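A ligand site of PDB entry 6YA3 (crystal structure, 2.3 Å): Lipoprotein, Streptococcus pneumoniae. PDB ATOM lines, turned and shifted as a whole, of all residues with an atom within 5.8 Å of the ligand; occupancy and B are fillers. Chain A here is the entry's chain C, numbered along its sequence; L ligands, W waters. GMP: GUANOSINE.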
ATOM      1  N   ASP A  26      -5.663 -27.415 -17.757  1.00  0.00           N
ATOM      2  CA  ASP A  26      -6.100 -28.721 -18.304  1.00  0.00           C
ATOM      3  C   ASP A  26      -5.194 -29.830 -17.746  1.00  0.00           C
ATOM      4  O   ASP A  26      -4.416 -29.570 -16.812  1.00  0.00           O
ATOM      5  CB  ASP A  26      -6.082 -28.633 -19.825  1.00  0.00           C
ATOM      6  CG  ASP A  26      -7.149 -29.442 -20.514  1.00  0.00           C
ATOM      7  OD1 ASP A  26      -7.694 -30.340 -19.861  1.00  0.00           O
ATOM      8  OD2 ASP A  26      -7.394 -29.162 -21.702  1.00  0.00           O
ATOM      9  N   THR A  27      -5.238 -31.016 -18.334  1.00  0.00           N
ATOM     10  CA  THR A  27      -4.517 -32.211 -17.820  1.00  0.00           C
ATOM     11  C   THR A  27      -3.000 -31.998 -17.935  1.00  0.00           C
ATOM     12  O   THR A  27      -2.302 -32.430 -16.986  1.00  0.00           O
ATOM     13  CB  THR A  27      -5.000 -33.524 -18.459  1.00  0.00           C
ATOM     14  OG1 THR A  27      -6.274 -33.383 -19.098  1.00  0.00           O
ATOM     15  CG2 THR A  27      -5.069 -34.629 -17.428  1.00  0.00           C
ATOM     16  N   GLY A  28      -2.516 -31.336 -18.999  1.00  0.00           N
ATOM     17  CA  GLY A  28      -1.093 -31.010 -19.241  1.00  0.00           C
ATOM     18  C   GLY A  28      -0.306 -30.593 -18.001  1.00  0.00           C
ATOM     19  O   GLY A  28       0.847 -31.071 -17.830  1.00  0.00           O
ATOM     20  N   GLY A  29      -0.906 -29.724 -17.173  1.00  0.00           N
ATOM     21  CA  GLY A  29      -0.334 -29.216 -15.902  1.00  0.00           C
ATOM     22  C   GLY A  29       0.548 -27.986 -16.104  1.00  0.00           C
ATOM     23  O   GLY A  29       1.080 -27.811 -17.199  1.00  0.00           O
ATOM     24  N   ASP A  32       4.250 -28.311 -17.789  1.00  0.00           N
ATOM     25  CA  ASP A  32       4.259 -28.915 -19.156  1.00  0.00           C
ATOM     26  C   ASP A  32       5.395 -28.320 -20.007  1.00  0.00           C
ATOM     27  O   ASP A  32       5.492 -28.727 -21.161  1.00  0.00           O
ATOM     28  CB  ASP A  32       2.894 -28.743 -19.825  1.00  0.00           C
ATOM     29  CG  ASP A  32       2.504 -27.309 -20.202  1.00  0.00           C
ATOM     30  OD1 ASP A  32       3.305 -26.386 -19.932  1.00  0.00           O
ATOM     31  OD2 ASP A  32       1.382 -27.136 -20.784  1.00  0.00           O
ATOM     32  N   SER A  34       5.497 -25.823 -21.524  1.00  0.00           N
ATOM     33  CA  SER A  34       4.966 -25.166 -22.731  1.00  0.00           C
ATOM     34  C   SER A  34       3.780 -24.271 -22.419  1.00  0.00           C
ATOM     35  O   SER A  34       3.965 -23.323 -21.730  1.00  0.00           O
ATOM     36  CB  SER A  34       4.688 -26.140 -23.852  1.00  0.00           C
ATOM     37  OG  SER A  34       4.044 -27.310 -23.409  1.00  0.00           O
ATOM     38  N   PHE A  35       2.622 -24.641 -22.955  1.00  0.00           N
ATOM     39  CA  PHE A  35       1.326 -23.918 -22.935  1.00  0.00           C
ATOM     40  C   PHE A  35       0.854 -23.479 -21.541  1.00  0.00           C
ATOM     41  O   PHE A  35       0.735 -22.307 -21.323  1.00  0.00           O
ATOM     42  CB  PHE A  35       0.272 -24.725 -23.710  1.00  0.00           C
ATOM     43  CG  PHE A  35      -1.069 -24.075 -23.854  1.00  0.00           C
ATOM     44  CD1 PHE A  35      -1.231 -22.925 -24.587  1.00  0.00           C
ATOM     45  CD2 PHE A  35      -2.181 -24.638 -23.269  1.00  0.00           C
ATOM     46  CE1 PHE A  35      -2.472 -22.347 -24.734  1.00  0.00           C
ATOM     47  CE2 PHE A  35      -3.433 -24.064 -23.431  1.00  0.00           C
ATOM     48  CZ  PHE A  35      -3.557 -22.914 -24.143  1.00  0.00           C
ATOM     49  N   ASN A  36       0.573 -24.436 -20.673  1.00  0.00           N
ATOM     50  CA  ASN A  36       0.058 -24.145 -19.309  1.00  0.00           C
ATOM     51  C   ASN A  36       1.156 -23.477 -18.491  1.00  0.00           C
ATOM     52  O   ASN A  36       0.849 -22.552 -17.753  1.00  0.00           O
ATOM     53  CB  ASN A  36      -0.481 -25.398 -18.617  1.00  0.00           C
ATOM     54  CG  ASN A  36      -1.685 -25.996 -19.312  1.00  0.00           C
ATOM     55  OD1 ASN A  36      -2.749 -25.397 -19.289  1.00  0.00           O
ATOM     56  ND2 ASN A  36      -1.518 -27.150 -19.937  1.00  0.00           N
ATOM     57  N   VAL A  86      -7.700 -22.097 -19.451  1.00  0.00           N
ATOM     58  CA  VAL A  86      -6.513 -22.282 -20.334  1.00  0.00           C
ATOM     59  C   VAL A  86      -6.718 -23.532 -21.180  1.00  0.00           C
ATOM     60  O   VAL A  86      -6.461 -24.621 -20.684  1.00  0.00           O
ATOM     61  CB  VAL A  86      -5.207 -22.348 -19.535  1.00  0.00           C
ATOM     62  CG1 VAL A  86      -4.022 -22.236 -20.484  1.00  0.00           C
ATOM     63  CG2 VAL A  86      -5.153 -21.275 -18.468  1.00  0.00           C
ATOM     64  N   GLY A  87      -7.107 -23.350 -22.441  1.00  0.00           N
ATOM     65  CA  GLY A  87      -7.245 -24.465 -23.398  1.00  0.00           C
ATOM     66  C   GLY A  87      -8.647 -24.515 -23.981  1.00  0.00           C
ATOM     67  O   GLY A  87      -9.592 -24.153 -23.272  1.00  0.00           O
ATOM     68  N   PHE A  88      -8.781 -24.955 -25.236  1.00  0.00           N
ATOM     69  CA  PHE A  88     -10.078 -25.013 -25.957  1.00  0.00           C
ATOM     70  C   PHE A  88     -11.092 -25.913 -25.215  1.00  0.00           C
ATOM     71  O   PHE A  88     -12.284 -25.610 -25.298  1.00  0.00           O
ATOM     72  CB  PHE A  88      -9.882 -25.438 -27.420  1.00  0.00           C
ATOM     73  CG  PHE A  88      -9.420 -26.856 -27.620  1.00  0.00           C
ATOM     74  CD1 PHE A  88     -10.326 -27.909 -27.612  1.00  0.00           C
ATOM     75  CD2 PHE A  88      -8.073 -27.144 -27.844  1.00  0.00           C
ATOM     76  CE1 PHE A  88      -9.898 -29.219 -27.791  1.00  0.00           C
ATOM     77  CE2 PHE A  88      -7.647 -28.447 -28.010  1.00  0.00           C
ATOM     78  CZ  PHE A  88      -8.566 -29.484 -27.973  1.00  0.00           C
ATOM     79  N   ALA A  89     -10.625 -26.921 -24.476  1.00  0.00           N
ATOM     80  CA  ALA A  89     -11.471 -27.937 -23.800  1.00  0.00           C
ATOM     81  C   ALA A  89     -12.338 -27.292 -22.716  1.00  0.00           C
ATOM     82  O   ALA A  89     -13.401 -27.867 -22.380  1.00  0.00           O
ATOM     83  CB  ALA A  89     -10.599 -29.038 -23.243  1.00  0.00           C
ATOM     84  N   ASP A 110      -7.344 -19.964 -26.369  1.00  0.00           N
ATOM     85  CA  ASP A 110      -7.305 -20.915 -27.513  1.00  0.00           C
ATOM     86  C   ASP A 110      -8.681 -21.254 -28.101  1.00  0.00           C
ATOM     87  O   ASP A 110      -8.720 -22.157 -28.883  1.00  0.00           O
ATOM     88  CB  ASP A 110      -6.471 -22.163 -27.256  1.00  0.00           C
ATOM     89  CG  ASP A 110      -5.071 -22.079 -27.797  1.00  0.00           C
ATOM     90  OD1 ASP A 110      -4.764 -21.108 -28.421  1.00  0.00           O
ATOM     91  OD2 ASP A 110      -4.350 -23.003 -27.583  1.00  0.00           O
ATOM     92  N   ASP A 126      -1.248 -19.760 -34.843  1.00  0.00           N
ATOM     93  CA  ASP A 126      -0.214 -20.816 -34.671  1.00  0.00           C
ATOM     94  C   ASP A 126       0.132 -21.427 -36.042  1.00  0.00           C
ATOM     95  O   ASP A 126       1.229 -22.013 -36.193  1.00  0.00           O
ATOM     96  CB  ASP A 126      -0.705 -21.870 -33.687  1.00  0.00           C
ATOM     97  CG  ASP A 126      -0.974 -21.359 -32.270  1.00  0.00           C
ATOM     98  OD1 ASP A 126      -0.030 -20.753 -31.678  1.00  0.00           O
ATOM     99  OD2 ASP A 126      -2.118 -21.585 -31.753  1.00  0.00           O
ATOM    100  N   VAL A 156      -7.612 -26.061 -33.290  1.00  0.00           N
ATOM    101  CA  VAL A 156      -6.378 -25.419 -32.755  1.00  0.00           C
ATOM    102  C   VAL A 156      -5.152 -26.144 -33.294  1.00  0.00           C
ATOM    103  O   VAL A 156      -4.263 -25.472 -33.859  1.00  0.00           O
ATOM    104  CB  VAL A 156      -6.381 -25.369 -31.219  1.00  0.00           C
ATOM    105  CG1 VAL A 156      -5.032 -24.947 -30.685  1.00  0.00           C
ATOM    106  CG2 VAL A 156      -7.459 -24.439 -30.692  1.00  0.00           C
ATOM    107  N   ILE A 157      -5.087 -27.462 -33.115  1.00  0.00           N
ATOM    108  CA  ILE A 157      -3.878 -28.234 -33.516  1.00  0.00           C
ATOM    109  C   ILE A 157      -3.824 -28.370 -35.040  1.00  0.00           C
ATOM    110  O   ILE A 157      -2.698 -28.391 -35.568  1.00  0.00           O
ATOM    111  CB  ILE A 157      -3.799 -29.596 -32.803  1.00  0.00           C
ATOM    112  CG1 ILE A 157      -3.925 -29.469 -31.286  1.00  0.00           C
ATOM    113  CG2 ILE A 157      -2.510 -30.318 -33.199  1.00  0.00           C
ATOM    114  CD1 ILE A 157      -2.820 -28.649 -30.629  1.00  0.00           C
ATOM    115  N   PHE A 160      -1.806 -25.536 -36.452  1.00  0.00           N
ATOM    116  CA  PHE A 160      -0.342 -25.787 -36.404  1.00  0.00           C
ATOM    117  C   PHE A 160       0.047 -26.716 -37.557  1.00  0.00           C
ATOM    118  O   PHE A 160       1.048 -26.452 -38.220  1.00  0.00           O
ATOM    119  CB  PHE A 160       0.070 -26.463 -35.105  1.00  0.00           C
ATOM    120  CG  PHE A 160       0.249 -25.599 -33.882  1.00  0.00           C
ATOM    121  CD1 PHE A 160       1.492 -25.113 -33.540  1.00  0.00           C
ATOM    122  CD2 PHE A 160      -0.796 -25.392 -32.995  1.00  0.00           C
ATOM    123  CE1 PHE A 160       1.677 -24.398 -32.371  1.00  0.00           C
ATOM    124  CE2 PHE A 160      -0.620 -24.657 -31.837  1.00  0.00           C
ATOM    125  CZ  PHE A 160       0.618 -24.163 -31.531  1.00  0.00           C
ATOM    126  N   PHE A 185      -3.003 -34.087 -24.069  1.00  0.00           N
ATOM    127  CA  PHE A 185      -1.946 -33.084 -23.780  1.00  0.00           C
ATOM    128  C   PHE A 185      -1.192 -33.448 -22.497  1.00  0.00           C
ATOM    129  O   PHE A 185      -0.230 -32.743 -22.173  1.00  0.00           O
ATOM    130  CB  PHE A 185      -2.537 -31.677 -23.724  1.00  0.00           C
ATOM    131  CG  PHE A 185      -3.119 -31.190 -25.038  1.00  0.00           C
ATOM    132  CD1 PHE A 185      -2.286 -30.818 -26.078  1.00  0.00           C
ATOM    133  CD2 PHE A 185      -4.482 -31.081 -25.223  1.00  0.00           C
ATOM    134  CE1 PHE A 185      -2.804 -30.363 -27.278  1.00  0.00           C
ATOM    135  CE2 PHE A 185      -5.008 -30.607 -26.410  1.00  0.00           C
ATOM    136  CZ  PHE A 185      -4.164 -30.261 -27.451  1.00  0.00           C
ATOM    137  N   GLN A 208       6.729 -31.324 -32.023  1.00  0.00           N
ATOM    138  CA  GLN A 208       5.738 -31.802 -31.030  1.00  0.00           C
ATOM    139  C   GLN A 208       4.790 -30.668 -30.653  1.00  0.00           C
ATOM    140  O   GLN A 208       5.259 -29.694 -30.128  1.00  0.00           O
ATOM    141  CB  GLN A 208       6.406 -32.499 -29.837  1.00  0.00           C
ATOM    142  CG  GLN A 208       7.673 -31.874 -29.296  1.00  0.00           C
ATOM    143  CD  GLN A 208       7.439 -30.769 -28.292  1.00  0.00           C
ATOM    144  OE1 GLN A 208       6.789 -30.944 -27.287  1.00  0.00           O
ATOM    145  NE2 GLN A 208       7.967 -29.604 -28.584  1.00  0.00           N
ATOM    146  N   VAL A 209       3.503 -30.854 -30.902  1.00  0.00           N
ATOM    147  CA  VAL A 209       2.426 -29.855 -30.647  1.00  0.00           C
ATOM    148  C   VAL A 209       1.378 -30.596 -29.821  1.00  0.00           C
ATOM    149  O   VAL A 209       0.281 -30.796 -30.296  1.00  0.00           O
ATOM    150  CB  VAL A 209       1.839 -29.316 -31.972  1.00  0.00           C
ATOM    151  CG1 VAL A 209       0.913 -28.133 -31.750  1.00  0.00           C
ATOM    152  CG2 VAL A 209       2.927 -28.973 -32.962  1.00  0.00           C
ATOM    153  N   ALA A 210       1.762 -30.932 -28.606  1.00  0.00           N
ATOM    154  CA  ALA A 210       0.938 -31.771 -27.726  1.00  0.00           C
ATOM    155  C   ALA A 210       1.204 -31.438 -26.261  1.00  0.00           C
ATOM    156  O   ALA A 210       1.053 -32.311 -25.460  1.00  0.00           O
ATOM    157  CB  ALA A 210       1.282 -33.205 -28.026  1.00  0.00           C
ATOM    158  N   GLY A 211       1.602 -30.198 -25.958  1.00  0.00           N
ATOM    159  CA  GLY A 211       1.873 -29.742 -24.592  1.00  0.00           C
ATOM    160  C   GLY A 211       2.761 -30.730 -23.850  1.00  0.00           C
ATOM    161  O   GLY A 211       3.816 -31.066 -24.393  1.00  0.00           O
ATOM    162  N   GLY A 212       2.330 -31.196 -22.673  1.00  0.00           N
ATOM    163  CA  GLY A 212       3.114 -32.060 -21.762  1.00  0.00           C
ATOM    164  C   GLY A 212       3.388 -33.439 -22.354  1.00  0.00           C
ATOM    165  O   GLY A 212       4.416 -34.038 -21.970  1.00  0.00           O
ATOM    166  N   VAL A 239       7.883 -26.026 -28.720  1.00  0.00           N
ATOM    167  CA  VAL A 239       6.530 -25.440 -28.913  1.00  0.00           C
ATOM    168  C   VAL A 239       6.198 -24.551 -27.716  1.00  0.00           C
ATOM    169  O   VAL A 239       6.580 -24.921 -26.603  1.00  0.00           O
ATOM    170  CB  VAL A 239       5.499 -26.567 -29.137  1.00  0.00           C
ATOM    171  CG1 VAL A 239       5.192 -27.332 -27.857  1.00  0.00           C
ATOM    172  CG2 VAL A 239       4.232 -26.037 -29.758  1.00  0.00           C
ATOM    173  N   ASP A 240       5.520 -23.427 -27.989  1.00  0.00           N
ATOM    174  CA  ASP A 240       4.887 -22.495 -27.014  1.00  0.00           C
ATOM    175  C   ASP A 240       5.963 -21.676 -26.297  1.00  0.00           C
ATOM    176  O   ASP A 240       5.906 -20.452 -26.405  1.00  0.00           O
ATOM    177  CB  ASP A 240       3.966 -23.235 -26.040  1.00  0.00           C
ATOM    178  CG  ASP A 240       2.846 -24.022 -26.709  1.00  0.00           C
ATOM    179  OD1 ASP A 240       2.321 -23.553 -27.781  1.00  0.00           O
ATOM    180  OD2 ASP A 240       2.507 -25.117 -26.180  1.00  0.00           O
ATOM    181  N   LYS A 266       4.454 -18.966 -28.377  1.00  0.00           N
ATOM    182  CA  LYS A 266       3.038 -18.582 -28.204  1.00  0.00           C
ATOM    183  C   LYS A 266       3.011 -17.814 -26.881  1.00  0.00           C
ATOM    184  O   LYS A 266       3.247 -18.436 -25.860  1.00  0.00           O
ATOM    185  CB  LYS A 266       2.175 -19.839 -28.225  1.00  0.00           C
ATOM    186  CG  LYS A 266       0.670 -19.632 -28.218  1.00  0.00           C
ATOM    187  CD  LYS A 266      -0.044 -20.950 -28.344  1.00  0.00           C
ATOM    188  CE  LYS A 266      -1.520 -20.845 -28.648  1.00  0.00           C
ATOM    189  NZ  LYS A 266      -2.078 -22.164 -29.066  1.00  0.00           N
HETATM  190  O5' GMP L   1       1.504 -27.386 -26.931  1.00  0.00           O
HETATM  191  C5' GMP L   1       1.082 -27.106 -28.269  1.00  0.00           C
HETATM  192  C4' GMP L   1      -0.313 -26.524 -28.316  1.00  0.00           C
HETATM  193  O4' GMP L   1      -1.248 -27.500 -27.802  1.00  0.00           O
HETATM  194  C3' GMP L   1      -0.552 -25.292 -27.431  1.00  0.00           C
HETATM  195  O3' GMP L   1      -0.235 -24.061 -28.069  1.00  0.00           O
HETATM  196  C2' GMP L   1      -2.053 -25.372 -27.211  1.00  0.00           C
HETATM  197  O2' GMP L   1      -2.829 -24.981 -28.320  1.00  0.00           O
HETATM  198  C1' GMP L   1      -2.268 -26.864 -27.073  1.00  0.00           C
HETATM  199  N9  GMP L   1      -2.242 -27.342 -25.696  1.00  0.00           N
HETATM  200  C8  GMP L   1      -1.152 -27.639 -24.931  1.00  0.00           C
HETATM  201  N7  GMP L   1      -1.451 -28.073 -23.733  1.00  0.00           N
HETATM  202  C5  GMP L   1      -2.835 -28.068 -23.711  1.00  0.00           C
HETATM  203  C6  GMP L   1      -3.713 -28.453 -22.673  1.00  0.00           C
HETATM  204  O6  GMP L   1      -3.426 -28.850 -21.547  1.00  0.00           O
HETATM  205  N1  GMP L   1      -5.039 -28.339 -23.076  1.00  0.00           N
HETATM  206  C2  GMP L   1      -5.473 -27.893 -24.298  1.00  0.00           C
HETATM  207  N2  GMP L   1      -6.800 -27.838 -24.482  1.00  0.00           N
HETATM  208  N3  GMP L   1      -4.647 -27.511 -25.272  1.00  0.00           N
HETATM  209  C4  GMP L   1      -3.341 -27.640 -24.912  1.00  0.00           C
HETATM  210  O   HOH W   1       0.156 -29.296 -21.768  1.00  0.00           O
HETATM  211  O   HOH W   2      -5.898 -25.179 -26.399  1.00  0.00           O
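The backbone carbonyl oxygen (O) of Asp 240 is in hydrogen-bond range of the backbone NH (N) of Lys 266 (2.9 Å). The backbone NH (N) of Phe 35 sits at hydrogen-bond distance from the side-chain carboxylate (OD2) of Asp 240 (3.3 Å). The side-chain amino group (NZ) of Lys 266 lies within salt-bridge range of the side-chain carboxylate (OD2) of Asp 110 (2.8 Å). OD2 of Asp 126 is in salt-bridge range of NZ of Lys 266, at 2.7 Å. OG1 of Thr 27 sits at hydrogen-bond distance from OD1 of Asp 26, 3.4 Å away. The backbone NH (N) of Asn 36 is in hydrogen-bond range of the side-chain carboxylate (OD2) of Asp 32, 2.8 Å away. The backbone carbonyl oxygen (O) of Phe 185 lies within hydrogen-bond range of the backbone NH (N) of Gly 212.
Water W2 lies within hydrogen-bond range of a nitrogen (N3) of the ligand, the side-chain carboxylate of Asp 110 and the backbone NH of Phe 88.
OD2 of Asp 240 is in hydrogen-bond range of O5' of the ligand, 2.6 Å away. OD2 of Asp 110 lies within hydrogen-bond range of O2' of the ligand (2.6 Å). NZ of Lys 266 lies within hydrogen-bond range of O3' of the ligand. OD2 of Asp 26 is in hydrogen-bond range of N1 of the ligand, at 2.8 Å. N of Gly 211 is in hydrogen-bond range of O5' of the ligand. The side-chain amide nitrogen of Asn 36 is in hydrogen-bond range of an oxygen (O6) of the ligand.
Merely in contact with the ligand: Val 156 (3.2 Å), Phe 185 (3.3 Å), Ile 157 (3.4 Å), Phe 35 (3.5 Å), Phe 160 (3.6 Å), Gly 87 (3.6 Å), Phe 88 (3.6 Å), Val 209 (3.6 Å), Val 239 (3.6 Å), Gly 28 (3.7 Å), Ala 210 (3.9 Å) and Ala 89 (3.9 Å). Hydrophobic or aromatic side chains within 4 Å of the ligand: Phe 35, Phe 88, Val 156, Ile 157, Phe 160, Phe 185, Val 209 and Val 239.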
